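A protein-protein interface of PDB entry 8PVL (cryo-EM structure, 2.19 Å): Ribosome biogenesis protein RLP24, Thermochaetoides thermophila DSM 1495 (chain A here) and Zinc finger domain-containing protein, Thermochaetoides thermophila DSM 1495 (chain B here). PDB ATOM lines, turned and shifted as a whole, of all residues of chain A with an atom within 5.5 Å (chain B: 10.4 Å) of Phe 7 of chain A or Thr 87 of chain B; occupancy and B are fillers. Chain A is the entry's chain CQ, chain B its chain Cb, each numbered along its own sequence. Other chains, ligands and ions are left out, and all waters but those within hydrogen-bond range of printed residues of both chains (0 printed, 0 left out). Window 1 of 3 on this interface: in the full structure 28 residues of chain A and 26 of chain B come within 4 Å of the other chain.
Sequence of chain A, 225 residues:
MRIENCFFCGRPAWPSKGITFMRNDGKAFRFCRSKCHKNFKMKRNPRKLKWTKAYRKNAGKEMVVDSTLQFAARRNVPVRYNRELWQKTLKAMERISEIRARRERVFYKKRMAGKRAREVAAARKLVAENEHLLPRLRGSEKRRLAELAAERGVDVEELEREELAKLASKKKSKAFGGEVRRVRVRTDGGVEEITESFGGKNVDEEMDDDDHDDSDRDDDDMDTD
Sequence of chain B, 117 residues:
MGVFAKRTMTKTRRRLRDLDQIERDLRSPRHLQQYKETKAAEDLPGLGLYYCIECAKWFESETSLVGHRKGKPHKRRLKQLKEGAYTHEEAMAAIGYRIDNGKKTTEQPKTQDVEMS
Asn 5 of chain A touches Ile 95 of chain B. Thr 87 of chain B touches Phe 7 of chain A (C to CE1, 3.7 Å). His 88 of chain B touches Phe 7 of chain A (ND1 to CE1, 3.6 Å). Phe 7 of chain A touches Ala 91 of chain B (O to CB, 3.8 Å). O of Phe 8 of chain A touches OH of Tyr 86 of chain B (3.7 Å). Ile 95 of chain B touches Gly 10 of chain A (CG2 to O, 3.6 Å). His 88 of chain B touches Phe 29 of chain A. CG of Pro 46 of chain A touches CD2 of Tyr 86 of chain B, at 3.6 Å.
Among the printed residues, 9 pairs touch across the chains. Among the printed residues, no Asp or Glu carboxylate lies within 4 Å of a Lys or Arg side-chain nitrogen of the other chain.
The side-chain hydroxyl of Thr 87 of chain B lies close to the side-chain carboxylate of Glu 89 of chain B (3.4 Å). SG of Cys 6 of chain A sits close to N of Phe 8 of chain A (3.4 Å). The backbone NH of Phe 7 of chain A is in hydrogen-bond range of the backbone carbonyl oxygen of Arg 30 of chain A. OD1 of Asn 5 of chain A sits close to O of Gly 10 of chain A.
The side-chain hydroxyl (OH) of Tyr 86 of chain B is in hydrogen-bond range of the backbone carbonyl oxygen (O) of Phe 7 of chain A.
Phe 7 of chain A touches just these residues of chain B: Tyr 86, Thr 87, His 88 and Ala 91. Thr 87 of chain B touches just one residue of chain A: Phe 7. No residue of chain B comes within 4 Å of Cys 6 of chain A. Of chain B, only His 88 comes within 4 Å of Phe 29 of chain A. Printed residues of chain A within 4 Å of His 88 of chain B: Phe 7 and Phe 29. Printed residues of chain B within 4 Å of Phe 8 of chain A: Tyr 86. Of the printed residues of chain B, Gly 10 of chain A touches Ile 95. The nearest printed residue of chain A that does not touch Thr 87 of chain B is Phe 29 of chain A (6.4 Å). The nearest printed residue of chain A that does not touch Ala 91 of chain B is Cys 6 of chain A (5.3 Å).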
ATOM      1  N   ASN A   5      20.280   2.816  11.331  1.00  0.00           N
ATOM      2  CA  ASN A   5      19.468   2.542  12.503  1.00  0.00           C
ATOM      3  C   ASN A   5      19.648   3.663  13.511  1.00  0.00           C
ATOM      4  O   ASN A   5      20.718   4.269  13.603  1.00  0.00           O
ATOM      5  CB  ASN A   5      19.825   1.196  13.139  1.00  0.00           C
ATOM      6  CG  ASN A   5      19.178   0.029  12.425  1.00  0.00           C
ATOM      7  OD1 ASN A   5      18.133  -0.466  12.841  1.00  0.00           O
ATOM      8  ND2 ASN A   5      19.797  -0.414  11.340  1.00  0.00           N
ATOM      9  N   CYS A   6      18.583   3.944  14.254  1.00  0.00           N
ATOM     10  CA  CYS A   6      18.636   5.001  15.251  1.00  0.00           C
ATOM     11  C   CYS A   6      19.517   4.575  16.416  1.00  0.00           C
ATOM     12  O   CYS A   6      19.379   3.465  16.938  1.00  0.00           O
ATOM     13  CB  CYS A   6      17.233   5.345  15.745  1.00  0.00           C
ATOM     14  SG  CYS A   6      17.204   6.621  17.023  1.00  0.00           S
ATOM     15  N   PHE A   7      20.431   5.465  16.808  1.00  0.00           N
ATOM     16  CA  PHE A   7      21.317   5.199  17.936  1.00  0.00           C
ATOM     17  C   PHE A   7      20.526   5.035  19.226  1.00  0.00           C
ATOM     18  O   PHE A   7      20.812   4.144  20.032  1.00  0.00           O
ATOM     19  CB  PHE A   7      22.337   6.335  18.056  1.00  0.00           C
ATOM     20  CG  PHE A   7      23.115   6.340  19.342  1.00  0.00           C
ATOM     21  CD1 PHE A   7      24.226   5.528  19.498  1.00  0.00           C
ATOM     22  CD2 PHE A   7      22.763   7.191  20.380  1.00  0.00           C
ATOM     23  CE1 PHE A   7      24.950   5.539  20.672  1.00  0.00           C
ATOM     24  CE2 PHE A   7      23.485   7.205  21.557  1.00  0.00           C
ATOM     25  CZ  PHE A   7      24.581   6.380  21.700  1.00  0.00           C
ATOM     26  N   PHE A   8      19.516   5.877  19.428  1.00  0.00           N
ATOM     27  CA  PHE A   8      18.775   5.876  20.682  1.00  0.00           C
ATOM     28  C   PHE A   8      17.809   4.699  20.770  1.00  0.00           C
ATOM     29  O   PHE A   8      17.883   3.898  21.707  1.00  0.00           O
ATOM     30  CB  PHE A   8      18.025   7.197  20.834  1.00  0.00           C
ATOM     31  CG  PHE A   8      17.751   7.574  22.254  1.00  0.00           C
ATOM     32  CD1 PHE A   8      16.580   7.179  22.872  1.00  0.00           C
ATOM     33  CD2 PHE A   8      18.659   8.337  22.969  1.00  0.00           C
ATOM     34  CE1 PHE A   8      16.322   7.527  24.177  1.00  0.00           C
ATOM     35  CE2 PHE A   8      18.405   8.693  24.277  1.00  0.00           C
ATOM     36  CZ  PHE A   8      17.238   8.283  24.883  1.00  0.00           C
ATOM     37  N   CYS A   9      16.897   4.576  19.805  1.00  0.00           N
ATOM     38  CA  CYS A   9      15.824   3.595  19.888  1.00  0.00           C
ATOM     39  C   CYS A   9      16.015   2.374  18.999  1.00  0.00           C
ATOM     40  O   CYS A   9      15.399   1.341  19.269  1.00  0.00           O
ATOM     41  CB  CYS A   9      14.479   4.249  19.544  1.00  0.00           C
ATOM     42  SG  CYS A   9      14.207   4.482  17.784  1.00  0.00           S
ATOM     43  N   GLY A  10      16.834   2.462  17.954  1.00  0.00           N
ATOM     44  CA  GLY A  10      17.112   1.318  17.112  1.00  0.00           C
ATOM     45  C   GLY A  10      16.180   1.113  15.937  1.00  0.00           C
ATOM     46  O   GLY A  10      16.304   0.094  15.247  1.00  0.00           O
ATOM     47  N   PHE A  29      26.185  10.618  15.806  1.00  0.00           N
ATOM     48  CA  PHE A  29      25.018   9.996  16.426  1.00  0.00           C
ATOM     49  C   PHE A  29      23.813  10.258  15.535  1.00  0.00           C
ATOM     50  O   PHE A  29      23.333  11.391  15.460  1.00  0.00           O
ATOM     51  CB  PHE A  29      24.775  10.549  17.832  1.00  0.00           C
ATOM     52  CG  PHE A  29      25.895  10.288  18.796  1.00  0.00           C
ATOM     53  CD1 PHE A  29      26.984  11.145  18.867  1.00  0.00           C
ATOM     54  CD2 PHE A  29      25.853   9.194  19.642  1.00  0.00           C
ATOM     55  CE1 PHE A  29      28.012  10.905  19.755  1.00  0.00           C
ATOM     56  CE2 PHE A  29      26.878   8.951  20.533  1.00  0.00           C
ATOM     57  CZ  PHE A  29      27.959   9.808  20.590  1.00  0.00           C
ATOM     58  N   ARG A  30      23.323   9.220  14.867  1.00  0.00           N
ATOM     59  CA  ARG A  30      22.174   9.350  13.982  1.00  0.00           C
ATOM     60  C   ARG A  30      20.897   9.015  14.741  1.00  0.00           C
ATOM     61  O   ARG A  30      20.781   7.934  15.325  1.00  0.00           O
ATOM     62  CB  ARG A  30      22.331   8.435  12.768  1.00  0.00           C
ATOM     63  CG  ARG A  30      21.081   8.289  11.918  1.00  0.00           C
ATOM     64  CD  ARG A  30      20.715   9.591  11.230  1.00  0.00           C
ATOM     65  NE  ARG A  30      19.521   9.452  10.405  1.00  0.00           N
ATOM     66  CZ  ARG A  30      19.515   8.977   9.168  1.00  0.00           C
ATOM     67  NH1 ARG A  30      20.628   8.589   8.569  1.00  0.00           N
ATOM     68  NH2 ARG A  30      18.361   8.887   8.514  1.00  0.00           N
ATOM     69  N   PHE A  31      19.943   9.943  14.732  1.00  0.00           N
ATOM     70  CA  PHE A  31      18.648   9.758  15.363  1.00  0.00           C
ATOM     71  C   PHE A  31      17.570   9.759  14.293  1.00  0.00           C
ATOM     72  O   PHE A  31      17.620  10.557  13.351  1.00  0.00           O
ATOM     73  CB  PHE A  31      18.359  10.863  16.380  1.00  0.00           C
ATOM     74  CG  PHE A  31      19.462  11.073  17.364  1.00  0.00           C
ATOM     75  CD1 PHE A  31      19.596  10.237  18.457  1.00  0.00           C
ATOM     76  CD2 PHE A  31      20.371  12.101  17.193  1.00  0.00           C
ATOM     77  CE1 PHE A  31      20.616  10.424  19.360  1.00  0.00           C
ATOM     78  CE2 PHE A  31      21.391  12.293  18.091  1.00  0.00           C
ATOM     79  CZ  PHE A  31      21.515  11.454  19.173  1.00  0.00           C
ATOM     80  N   PHE A  40      17.962  12.305  23.929  1.00  0.00           N
ATOM     81  CA  PHE A  40      19.421  12.308  23.970  1.00  0.00           C
ATOM     82  C   PHE A  40      19.957  13.622  24.528  1.00  0.00           C
ATOM     83  O   PHE A  40      20.887  13.627  25.341  1.00  0.00           O
ATOM     84  CB  PHE A  40      19.971  12.057  22.568  1.00  0.00           C
ATOM     85  CG  PHE A  40      21.471  12.019  22.495  1.00  0.00           C
ATOM     86  CD1 PHE A  40      22.161  10.859  22.804  1.00  0.00           C
ATOM     87  CD2 PHE A  40      22.190  13.136  22.093  1.00  0.00           C
ATOM     88  CE1 PHE A  40      23.538  10.818  22.726  1.00  0.00           C
ATOM     89  CE2 PHE A  40      23.565  13.098  22.013  1.00  0.00           C
ATOM     90  CZ  PHE A  40      24.239  11.939  22.330  1.00  0.00           C
ATOM     91  N   PRO A  46      18.694   5.260  27.053  1.00  0.00           N
ATOM     92  CA  PRO A  46      17.862   4.353  26.243  1.00  0.00           C
ATOM     93  C   PRO A  46      17.677   2.986  26.869  1.00  0.00           C
ATOM     94  O   PRO A  46      16.627   2.362  26.672  1.00  0.00           O
ATOM     95  CB  PRO A  46      18.632   4.255  24.918  1.00  0.00           C
ATOM     96  CG  PRO A  46      19.540   5.419  24.901  1.00  0.00           C
ATOM     97  CD  PRO A  46      19.873   5.740  26.316  1.00  0.00           C
ATOM     98  N   ASP B  18      29.372  14.227  28.122  1.00  0.00           N
ATOM     99  CA  ASP B  18      28.610  12.988  28.088  1.00  0.00           C
ATOM    100  C   ASP B  18      29.224  11.909  28.981  1.00  0.00           C
ATOM    101  O   ASP B  18      30.421  11.915  29.299  1.00  0.00           O
ATOM    102  CB  ASP B  18      28.493  12.465  26.656  1.00  0.00           C
ATOM    103  CG  ASP B  18      27.513  13.262  25.822  1.00  0.00           C
ATOM    104  OD1 ASP B  18      26.475  13.685  26.369  1.00  0.00           O
ATOM    105  OD2 ASP B  18      27.777  13.464  24.617  1.00  0.00           O
ATOM    106  N   LEU B  19      28.371  10.954  29.362  1.00  0.00           N
ATOM    107  CA  LEU B  19      28.769   9.895  30.282  1.00  0.00           C
ATOM    108  C   LEU B  19      29.760   8.923  29.653  1.00  0.00           C
ATOM    109  O   LEU B  19      30.640   8.414  30.349  1.00  0.00           O
ATOM    110  CB  LEU B  19      27.537   9.143  30.778  1.00  0.00           C
ATOM    111  CG  LEU B  19      27.720   8.301  32.041  1.00  0.00           C
ATOM    112  CD1 LEU B  19      28.047   9.187  33.230  1.00  0.00           C
ATOM    113  CD2 LEU B  19      26.481   7.469  32.313  1.00  0.00           C
ATOM    114  N   ASP B  20      29.641   8.647  28.351  1.00  0.00           N
ATOM    115  CA  ASP B  20      30.615   7.767  27.709  1.00  0.00           C
ATOM    116  C   ASP B  20      31.977   8.442  27.598  1.00  0.00           C
ATOM    117  O   ASP B  20      33.017   7.787  27.746  1.00  0.00           O
ATOM    118  CB  ASP B  20      30.113   7.322  26.335  1.00  0.00           C
ATOM    119  CG  ASP B  20      29.569   8.467  25.513  1.00  0.00           C
ATOM    120  OD1 ASP B  20      28.815   9.289  26.069  1.00  0.00           O
ATOM    121  OD2 ASP B  20      29.895   8.545  24.312  1.00  0.00           O
ATOM    122  N   GLN B  21      31.989   9.755  27.354  1.00  0.00           N
ATOM    123  CA  GLN B  21      33.237  10.509  27.391  1.00  0.00           C
ATOM    124  C   GLN B  21      33.849  10.490  28.786  1.00  0.00           C
ATOM    125  O   GLN B  21      35.072  10.394  28.934  1.00  0.00           O
ATOM    126  CB  GLN B  21      32.999  11.947  26.932  1.00  0.00           C
ATOM    127  CG  GLN B  21      32.473  12.071  25.516  1.00  0.00           C
ATOM    128  CD  GLN B  21      32.298  13.513  25.088  1.00  0.00           C
ATOM    129  OE1 GLN B  21      31.416  14.215  25.577  1.00  0.00           O
ATOM    130  NE2 GLN B  21      33.144  13.963  24.169  1.00  0.00           N
ATOM    131  N   ILE B  22      33.011  10.572  29.822  1.00  0.00           N
ATOM    132  CA  ILE B  22      33.506  10.504  31.196  1.00  0.00           C
ATOM    133  C   ILE B  22      34.063   9.114  31.511  1.00  0.00           C
ATOM    134  O   ILE B  22      35.084   8.976  32.198  1.00  0.00           O
ATOM    135  CB  ILE B  22      32.383  10.929  32.162  1.00  0.00           C
ATOM    136  CG1 ILE B  22      32.195  12.443  32.083  1.00  0.00           C
ATOM    137  CG2 ILE B  22      32.670  10.506  33.593  1.00  0.00           C
ATOM    138  CD1 ILE B  22      30.959  12.940  32.761  1.00  0.00           C
ATOM    139  N   GLU B  23      33.410   8.066  30.996  1.00  0.00           N
ATOM    140  CA  GLU B  23      33.921   6.704  31.136  1.00  0.00           C
ATOM    141  C   GLU B  23      35.283   6.554  30.470  1.00  0.00           C
ATOM    142  O   GLU B  23      36.194   5.924  31.025  1.00  0.00           O
ATOM    143  CB  GLU B  23      32.931   5.713  30.525  1.00  0.00           C
ATOM    144  CG  GLU B  23      32.630   4.498  31.377  1.00  0.00           C
ATOM    145  CD  GLU B  23      31.516   3.649  30.794  1.00  0.00           C
ATOM    146  OE1 GLU B  23      31.242   3.779  29.583  1.00  0.00           O
ATOM    147  OE2 GLU B  23      30.911   2.856  31.545  1.00  0.00           O
ATOM    148  N   ARG B  24      35.438   7.132  29.278  1.00  0.00           N
ATOM    149  CA  ARG B  24      36.724   7.088  28.588  1.00  0.00           C
ATOM    150  C   ARG B  24      37.783   7.900  29.328  1.00  0.00           C
ATOM    151  O   ARG B  24      38.964   7.537  29.319  1.00  0.00           O
ATOM    152  CB  ARG B  24      36.556   7.586  27.154  1.00  0.00           C
ATOM    153  CG  ARG B  24      36.374   6.481  26.131  1.00  0.00           C
ATOM    154  CD  ARG B  24      36.088   7.044  24.747  1.00  0.00           C
ATOM    155  NE  ARG B  24      34.763   6.669  24.269  1.00  0.00           N
ATOM    156  CZ  ARG B  24      33.757   7.518  24.107  1.00  0.00           C
ATOM    157  NH1 ARG B  24      33.891   8.806  24.374  1.00  0.00           N
ATOM    158  NH2 ARG B  24      32.587   7.062  23.667  1.00  0.00           N
ATOM    159  N   ARG B  27      38.916   5.644  32.100  1.00  0.00           N
ATOM    160  CA  ARG B  27      39.730   4.528  31.627  1.00  0.00           C
ATOM    161  C   ARG B  27      41.115   4.973  31.163  1.00  0.00           C
ATOM    162  O   ARG B  27      42.111   4.309  31.468  1.00  0.00           O
ATOM    163  CB  ARG B  27      39.010   3.790  30.502  1.00  0.00           C
ATOM    164  CG  ARG B  27      38.288   2.538  30.961  1.00  0.00           C
ATOM    165  CD  ARG B  27      37.942   1.627  29.796  1.00  0.00           C
ATOM    166  NE  ARG B  27      38.049   2.303  28.509  1.00  0.00           N
ATOM    167  CZ  ARG B  27      37.015   2.669  27.766  1.00  0.00           C
ATOM    168  NH1 ARG B  27      35.770   2.465  28.166  1.00  0.00           N
ATOM    169  NH2 ARG B  27      37.233   3.256  26.594  1.00  0.00           N
ATOM    170  N   GLN B  80      25.349   5.725  37.778  1.00  0.00           N
ATOM    171  CA  GLN B  80      25.257   5.682  36.320  1.00  0.00           C
ATOM    172  C   GLN B  80      26.504   5.057  35.702  1.00  0.00           C
ATOM    173  O   GLN B  80      26.407   4.276  34.749  1.00  0.00           O
ATOM    174  CB  GLN B  80      25.039   7.089  35.768  1.00  0.00           C
ATOM    175  CG  GLN B  80      23.616   7.597  35.891  1.00  0.00           C
ATOM    176  CD  GLN B  80      23.497   9.067  35.550  1.00  0.00           C
ATOM    177  OE1 GLN B  80      24.498   9.755  35.365  1.00  0.00           O
ATOM    178  NE2 GLN B  80      22.267   9.555  35.468  1.00  0.00           N
ATOM    179  N   LEU B  81      27.681   5.382  36.239  1.00  0.00           N
ATOM    180  CA  LEU B  81      28.918   4.804  35.722  1.00  0.00           C
ATOM    181  C   LEU B  81      29.039   3.323  36.060  1.00  0.00           C
ATOM    182  O   LEU B  81      29.596   2.558  35.267  1.00  0.00           O
ATOM    183  CB  LEU B  81      30.120   5.574  36.263  1.00  0.00           C
ATOM    184  CG  LEU B  81      30.376   6.916  35.582  1.00  0.00           C
ATOM    185  CD1 LEU B  81      31.215   7.811  36.471  1.00  0.00           C
ATOM    186  CD2 LEU B  81      31.044   6.711  34.236  1.00  0.00           C
ATOM    187  N   GLU B  83      26.436   1.270  36.362  1.00  0.00           N
ATOM    188  CA  GLU B  83      25.550   0.639  35.388  1.00  0.00           C
ATOM    189  C   GLU B  83      26.152   0.647  33.989  1.00  0.00           C
ATOM    190  O   GLU B  83      25.864  -0.248  33.187  1.00  0.00           O
ATOM    191  CB  GLU B  83      24.189   1.333  35.378  1.00  0.00           C
ATOM    192  CG  GLU B  83      23.151   0.670  36.262  1.00  0.00           C
ATOM    193  CD  GLU B  83      22.197   1.667  36.885  1.00  0.00           C
ATOM    194  OE1 GLU B  83      22.364   2.881  36.646  1.00  0.00           O
ATOM    195  OE2 GLU B  83      21.277   1.235  37.612  1.00  0.00           O
ATOM    196  N   GLY B  84      26.980   1.630  33.682  1.00  0.00           N
ATOM    197  CA  GLY B  84      27.630   1.697  32.391  1.00  0.00           C
ATOM    198  C   GLY B  84      26.966   2.705  31.473  1.00  0.00           C
ATOM    199  O   GLY B  84      25.759   2.959  31.545  1.00  0.00           O
ATOM    200  N   ALA B  85      27.768   3.295  30.595  1.00  0.00           N
ATOM    201  CA  ALA B  85      27.254   4.277  29.657  1.00  0.00           C
ATOM    202  C   ALA B  85      26.775   3.604  28.378  1.00  0.00           C
ATOM    203  O   ALA B  85      27.327   2.594  27.934  1.00  0.00           O
ATOM    204  CB  ALA B  85      28.321   5.319  29.327  1.00  0.00           C
ATOM    205  N   TYR B  86      25.731   4.178  27.790  1.00  0.00           N
ATOM    206  CA  TYR B  86      25.194   3.685  26.531  1.00  0.00           C
ATOM    207  C   TYR B  86      26.128   4.080  25.395  1.00  0.00           C
ATOM    208  O   TYR B  86      26.502   5.250  25.269  1.00  0.00           O
ATOM    209  CB  TYR B  86      23.800   4.257  26.297  1.00  0.00           C
ATOM    210  CG  TYR B  86      23.081   3.662  25.114  1.00  0.00           C
ATOM    211  CD1 TYR B  86      22.652   2.345  25.134  1.00  0.00           C
ATOM    212  CD2 TYR B  86      22.843   4.412  23.974  1.00  0.00           C
ATOM    213  CE1 TYR B  86      21.997   1.799  24.057  1.00  0.00           C
ATOM    214  CE2 TYR B  86      22.189   3.873  22.892  1.00  0.00           C
ATOM    215  CZ  TYR B  86      21.765   2.566  22.940  1.00  0.00           C
ATOM    216  OH  TYR B  86      21.110   2.022  21.863  1.00  0.00           O
ATOM    217  N   THR B  87      26.509   3.108  24.571  1.00  0.00           N
ATOM    218  CA  THR B  87      27.497   3.323  23.525  1.00  0.00           C
ATOM    219  C   THR B  87      26.983   2.797  22.190  1.00  0.00           C
ATOM    220  O   THR B  87      25.922   2.173  22.101  1.00  0.00           O
ATOM    221  CB  THR B  87      28.834   2.648  23.867  1.00  0.00           C
ATOM    222  OG1 THR B  87      28.604   1.279  24.223  1.00  0.00           O
ATOM    223  CG2 THR B  87      29.529   3.364  25.017  1.00  0.00           C
ATOM    224  N   HIS B  88      27.772   3.059  21.145  1.00  0.00           N
ATOM    225  CA  HIS B  88      27.435   2.585  19.807  1.00  0.00           C
ATOM    226  C   HIS B  88      27.504   1.068  19.715  1.00  0.00           C
ATOM    227  O   HIS B  88      26.730   0.461  18.967  1.00  0.00           O
ATOM    228  CB  HIS B  88      28.365   3.215  18.773  1.00  0.00           C
ATOM    229  CG  HIS B  88      27.831   4.473  18.164  1.00  0.00           C
ATOM    230  ND1 HIS B  88      28.002   5.710  18.746  1.00  0.00           N
ATOM    231  CD2 HIS B  88      27.130   4.687  17.026  1.00  0.00           C
ATOM    232  CE1 HIS B  88      27.431   6.631  17.992  1.00  0.00           C
ATOM    233  NE2 HIS B  88      26.896   6.037  16.942  1.00  0.00           N
ATOM    234  N   GLU B  89      28.415   0.441  20.461  1.00  0.00           N
ATOM    235  CA  GLU B  89      28.511  -1.017  20.451  1.00  0.00           C
ATOM    236  C   GLU B  89      27.274  -1.653  21.076  1.00  0.00           C
ATOM    237  O   GLU B  89      26.750  -2.646  20.556  1.00  0.00           O
ATOM    238  CB  GLU B  89      29.782  -1.516  21.165  1.00  0.00           C
ATOM    239  CG  GLU B  89      31.204  -0.941  20.824  1.00  0.00           C
ATOM    240  CD  GLU B  89      31.349   0.574  20.735  1.00  0.00           C
ATOM    241  OE1 GLU B  89      30.852   1.278  21.637  1.00  0.00           O
ATOM    242  OE2 GLU B  89      31.961   1.055  19.758  1.00  0.00           O
ATOM    243  N   GLU B  90      26.781  -1.084  22.180  1.00  0.00           N
ATOM    244  CA  GLU B  90      25.545  -1.583  22.771  1.00  0.00           C
ATOM    245  C   GLU B  90      24.347  -1.282  21.876  1.00  0.00           C
ATOM    246  O   GLU B  90      23.419  -2.096  21.794  1.00  0.00           O
ATOM    247  CB  GLU B  90      25.358  -0.996  24.177  1.00  0.00           C
ATOM    248  CG  GLU B  90      23.931  -1.049  24.714  1.00  0.00           C
ATOM    249  CD  GLU B  90      23.854  -1.056  26.225  1.00  0.00           C
ATOM    250  OE1 GLU B  90      24.897  -1.272  26.872  1.00  0.00           O
ATOM    251  OE2 GLU B  90      22.746  -0.850  26.767  1.00  0.00           O
ATOM    252  N   ALA B  91      24.369  -0.144  21.174  1.00  0.00           N
ATOM    253  CA  ALA B  91      23.321   0.154  20.199  1.00  0.00           C
ATOM    254  C   ALA B  91      23.305  -0.870  19.068  1.00  0.00           C
ATOM    255  O   ALA B  91      22.238  -1.246  18.572  1.00  0.00           O
ATOM    256  CB  ALA B  91      23.513   1.563  19.640  1.00  0.00           C
ATOM    257  N   MET B  92      24.487  -1.311  18.638  1.00  0.00           N
ATOM    258  CA  MET B  92      24.599  -2.370  17.640  1.00  0.00           C
ATOM    259  C   MET B  92      24.057  -3.695  18.171  1.00  0.00           C
ATOM    260  O   MET B  92      23.297  -4.392  17.483  1.00  0.00           O
ATOM    261  CB  MET B  92      26.067  -2.508  17.237  1.00  0.00           C
ATOM    262  CG  MET B  92      26.316  -3.096  15.878  1.00  0.00           C
ATOM    263  SD  MET B  92      27.932  -2.634  15.232  1.00  0.00           S
ATOM    264  CE  MET B  92      27.533  -1.112  14.381  1.00  0.00           C
ATOM    265  N   ALA B  93      24.431  -4.049  19.403  1.00  0.00           N
ATOM    266  CA  ALA B  93      23.992  -5.307  19.997  1.00  0.00           C
ATOM    267  C   ALA B  93      22.498  -5.325  20.297  1.00  0.00           C
ATOM    268  O   ALA B  93      21.910  -6.409  20.372  1.00  0.00           O
ATOM    269  CB  ALA B  93      24.777  -5.586  21.277  1.00  0.00           C
ATOM    270  N   ALA B  94      21.882  -4.156  20.489  1.00  0.00           N
ATOM    271  CA  ALA B  94      20.447  -4.093  20.744  1.00  0.00           C
ATOM    272  C   ALA B  94      19.637  -4.557  19.542  1.00  0.00           C
ATOM    273  O   ALA B  94      18.611  -5.224  19.709  1.00  0.00           O
ATOM    274  CB  ALA B  94      20.042  -2.674  21.132  1.00  0.00           C
ATOM    275  N   ILE B  95      20.073  -4.209  18.331  1.00  0.00           N
ATOM    276  CA  ILE B  95      19.408  -4.656  17.116  1.00  0.00           C
ATOM    277  C   ILE B  95      20.032  -5.916  16.547  1.00  0.00           C
ATOM    278  O   ILE B  95      19.525  -6.452  15.553  1.00  0.00           O
ATOM    279  CB  ILE B  95      19.393  -3.545  16.049  1.00  0.00           C
ATOM    280  CG1 ILE B  95      20.818  -3.079  15.751  1.00  0.00           C
ATOM    281  CG2 ILE B  95      18.526  -2.386  16.504  1.00  0.00           C
ATOM    282  CD1 ILE B  95      20.926  -2.172  14.559  1.00  0.00           C
